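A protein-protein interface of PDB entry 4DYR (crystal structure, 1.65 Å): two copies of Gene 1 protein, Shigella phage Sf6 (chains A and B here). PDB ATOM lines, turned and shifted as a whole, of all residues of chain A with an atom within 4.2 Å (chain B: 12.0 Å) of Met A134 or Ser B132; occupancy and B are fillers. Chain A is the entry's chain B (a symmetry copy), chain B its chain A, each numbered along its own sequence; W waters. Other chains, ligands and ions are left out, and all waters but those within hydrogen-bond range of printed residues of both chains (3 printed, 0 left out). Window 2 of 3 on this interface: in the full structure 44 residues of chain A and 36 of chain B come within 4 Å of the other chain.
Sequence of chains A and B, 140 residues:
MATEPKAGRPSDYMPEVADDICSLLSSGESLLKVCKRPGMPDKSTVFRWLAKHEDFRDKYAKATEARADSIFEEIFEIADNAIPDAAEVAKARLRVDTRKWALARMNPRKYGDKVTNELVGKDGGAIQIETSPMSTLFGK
The backbone NH (N) of Ser A132 lies within hydrogen-bond range of the backbone carbonyl oxygen (O) of Ile B129 (2.9 Å).
The side-chain carboxylate (OE2) of Glu B130 is in hydrogen-bond range of the side-chain hydroxyl (OG) of Ser A135, at 2.8 Å.
OG of Ser B132 sits at hydrogen-bond distance from SD of Met A134, 2.9 Å away.
Among the printed residues, merely in contact across the chains: Ser A132 with Glu B130, Ser A132 with Thr B131, Pro A133 with Glu B130, Met A134 with Glu B130, Phe A138 with Glu B130 and Phe A138 with Ser B132.
Ser B132 touches just these residues of chain A: Met A134 and Phe A138.
Ser A135 touches just one residue of chain B: Glu B130 (2.8 Å).
No residue of chain B comes within 4 Å of Thr A136.
No residue of chain B comes within 4 Å of Gly A139.
Of the printed residues of chain A, Thr B131 touches Ser A132 (3.8 Å).
Of the printed residues of chain A, Glu B130 touches Ser A132, Pro A133, Met A134, Ser A135 and Phe A138.
The nearest printed residue of chain A that does not touch Ile B129 is Pro A133 (5.6 Å).
Among the printed residues, no Asp or Glu carboxylate lies within 4 Å of a Lys or Arg side-chain nitrogen of the other chain.
Position printed for both chains: 132.
Water W3 lies within hydrogen-bond range of OG of Ser A132 (2.5 Å), NE2 of Gln B128 (2.8 Å) and O of Ile B129 (3.2 Å).
Water W2 lies within hydrogen-bond range of the side-chain carboxylate of Glu B130 (2.8 Å), the side-chain hydroxyl of Thr A136 (2.8 Å) and the side-chain hydroxyl of Ser A135 (3.3 Å).
Water W1 bridges OE2 of Glu B130 (2.9 Å) and OG of Ser A135 (3.5 Å).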
ATOM      1  N   SER A 132      10.960  20.973  28.041  1.00  0.00           N
ATOM      2  CA  SER A 132       9.839  20.718  28.937  1.00  0.00           C
ATOM      3  C   SER A 132       9.493  19.239  28.923  1.00  0.00           C
ATOM      4  O   SER A 132       9.789  18.538  27.954  1.00  0.00           O
ATOM      5  CB  SER A 132       8.619  21.528  28.503  1.00  0.00           C
ATOM      6  OG  SER A 132       8.880  22.918  28.563  1.00  0.00           O
ATOM      7  N   PRO A 133       8.872  18.759  30.010  1.00  0.00           N
ATOM      8  CA  PRO A 133       8.372  17.384  30.077  1.00  0.00           C
ATOM      9  C   PRO A 133       7.439  17.125  28.903  1.00  0.00           C
ATOM     10  O   PRO A 133       6.752  18.048  28.453  1.00  0.00           O
ATOM     11  CB  PRO A 133       7.576  17.369  31.386  1.00  0.00           C
ATOM     12  CG  PRO A 133       8.190  18.442  32.220  1.00  0.00           C
ATOM     13  CD  PRO A 133       8.617  19.511  31.251  1.00  0.00           C
ATOM     14  N   MET A 134       7.420  15.900  28.391  1.00  0.00           N
ATOM     15  CA  MET A 134       6.510  15.601  27.299  1.00  0.00           C
ATOM     16  C   MET A 134       5.092  15.894  27.768  1.00  0.00           C
ATOM     17  O   MET A 134       4.754  15.668  28.933  1.00  0.00           O
ATOM     18  CB  MET A 134       6.673  14.163  26.799  1.00  0.00           C
ATOM     19  CG  MET A 134       6.482  13.094  27.842  1.00  0.00           C
ATOM     20  SD  MET A 134       7.087  11.506  27.230  1.00  0.00           S
ATOM     21  CE  MET A 134       6.110  11.296  25.741  1.00  0.00           C
ATOM     22  N   SER A 135       4.275  16.434  26.871  1.00  0.00           N
ATOM     23  CA  SER A 135       2.920  16.820  27.226  1.00  0.00           C
ATOM     24  C   SER A 135       1.891  15.910  26.564  1.00  0.00           C
ATOM     25  O   SER A 135       0.716  15.948  26.909  1.00  0.00           O
ATOM     26  CB  SER A 135       2.663  18.288  26.868  1.00  0.00           C
ATOM     27  OG  SER A 135       2.695  18.485  25.468  1.00  0.00           O
ATOM     28  N   THR A 136       2.343  15.098  25.610  1.00  0.00           N
ATOM     29  CA  THR A 136       1.496  14.097  24.965  1.00  0.00           C
ATOM     30  C   THR A 136       2.277  12.796  24.830  1.00  0.00           C
ATOM     31  O   THR A 136       3.502  12.799  24.902  1.00  0.00           O
ATOM     32  CB  THR A 136       1.059  14.552  23.570  1.00  0.00           C
ATOM     33  OG1 THR A 136       2.206  14.615  22.708  1.00  0.00           O
ATOM     34  CG2 THR A 136       0.410  15.924  23.640  1.00  0.00           C
ATOM     35  N   PHE A 138       3.933  10.733  22.839  1.00  0.00           N
ATOM     36  CA  PHE A 138       4.515  10.649  21.505  1.00  0.00           C
ATOM     37  C   PHE A 138       5.635   9.614  21.383  1.00  0.00           C
ATOM     38  O   PHE A 138       6.226   9.453  20.315  1.00  0.00           O
ATOM     39  CB  PHE A 138       4.981  12.028  21.005  1.00  0.00           C
ATOM     40  CG  PHE A 138       6.099  12.651  21.811  1.00  0.00           C
ATOM     41  CD1 PHE A 138       7.382  12.117  21.791  1.00  0.00           C
ATOM     42  CD2 PHE A 138       5.884  13.819  22.533  1.00  0.00           C
ATOM     43  CE1 PHE A 138       8.414  12.714  22.501  1.00  0.00           C
ATOM     44  CE2 PHE A 138       6.912  14.420  23.244  1.00  0.00           C
ATOM     45  CZ  PHE A 138       8.183  13.875  23.222  1.00  0.00           C
ATOM     46  N   GLY A 139       5.912   8.913  22.479  1.00  0.00           N
ATOM     47  CA  GLY A 139       6.984   7.932  22.513  1.00  0.00           C
ATOM     48  C   GLY A 139       6.659   6.638  21.791  1.00  0.00           C
ATOM     49  O   GLY A 139       5.586   6.479  21.200  1.00  0.00           O
ATOM     50  N   GLN B 128      10.864  25.585  21.566  1.00  0.00           N
ATOM     51  CA  GLN B 128      10.290  24.662  22.546  1.00  0.00           C
ATOM     52  C   GLN B 128      10.554  23.196  22.195  1.00  0.00           C
ATOM     53  O   GLN B 128      10.173  22.737  21.127  1.00  0.00           O
ATOM     54  CB  GLN B 128       8.774  24.902  22.678  1.00  0.00           C
ATOM     55  CG  GLN B 128       8.400  26.334  23.102  1.00  0.00           C
ATOM     56  CD  GLN B 128       8.920  26.678  24.482  1.00  0.00           C
ATOM     57  OE1 GLN B 128       9.534  27.725  24.687  1.00  0.00           O
ATOM     58  NE2 GLN B 128       8.671  25.798  25.439  1.00  0.00           N
ATOM     59  N   ILE B 129      11.201  22.458  23.095  1.00  0.00           N
ATOM     60  CA  ILE B 129      11.475  21.054  22.850  1.00  0.00           C
ATOM     61  C   ILE B 129      10.901  20.221  23.984  1.00  0.00           C
ATOM     62  O   ILE B 129      10.954  20.622  25.140  1.00  0.00           O
ATOM     63  CB  ILE B 129      12.988  20.800  22.746  1.00  0.00           C
ATOM     64  CG1 ILE B 129      13.544  21.507  21.505  1.00  0.00           C
ATOM     65  CG2 ILE B 129      13.288  19.306  22.670  1.00  0.00           C
ATOM     66  CD1 ILE B 129      15.058  21.381  21.337  1.00  0.00           C
ATOM     67  N   GLU B 130      10.323  19.078  23.636  1.00  0.00           N
ATOM     68  CA  GLU B 130       9.932  18.079  24.621  1.00  0.00           C
ATOM     69  C   GLU B 130      10.721  16.821  24.324  1.00  0.00           C
ATOM     70  O   GLU B 130      10.828  16.428  23.167  1.00  0.00           O
ATOM     71  CB  GLU B 130       8.432  17.781  24.520  1.00  0.00           C
ATOM     72  CG  GLU B 130       7.556  18.893  25.043  1.00  0.00           C
ATOM     73  CD  GLU B 130       6.074  18.594  24.902  1.00  0.00           C
ATOM     74  OE1 GLU B 130       5.720  17.424  24.624  1.00  0.00           O
ATOM     75  OE2 GLU B 130       5.268  19.536  25.073  1.00  0.00           O
ATOM     76  N   THR B 131      11.267  16.180  25.355  1.00  0.00           N
ATOM     77  CA  THR B 131      12.030  14.944  25.149  1.00  0.00           C
ATOM     78  C   THR B 131      11.433  13.726  25.858  1.00  0.00           C
ATOM     79  O   THR B 131      10.897  13.833  26.960  1.00  0.00           O
ATOM     80  CB  THR B 131      13.499  15.108  25.596  1.00  0.00           C
ATOM     81  OG1 THR B 131      14.095  16.197  24.880  1.00  0.00           O
ATOM     82  CG2 THR B 131      14.288  13.845  25.303  1.00  0.00           C
ATOM     83  N   SER B 132      11.541  12.571  25.206  1.00  0.00           N
ATOM     84  CA  SER B 132      11.138  11.294  25.785  1.00  0.00           C
ATOM     85  C   SER B 132      12.297  10.314  25.714  1.00  0.00           C
ATOM     86  O   SER B 132      12.866  10.108  24.641  1.00  0.00           O
ATOM     87  CB  SER B 132       9.960  10.705  25.014  1.00  0.00           C
ATOM     88  OG  SER B 132       8.870  11.606  24.988  1.00  0.00           O
HETATM   89  O   HOH W   1       3.691  20.597  22.900  1.00  0.00           O
HETATM   90  O   HOH W   2       3.739  17.017  22.677  1.00  0.00           O
HETATM   91  O   HOH W   3       9.327  23.176  26.081  1.00  0.00           O
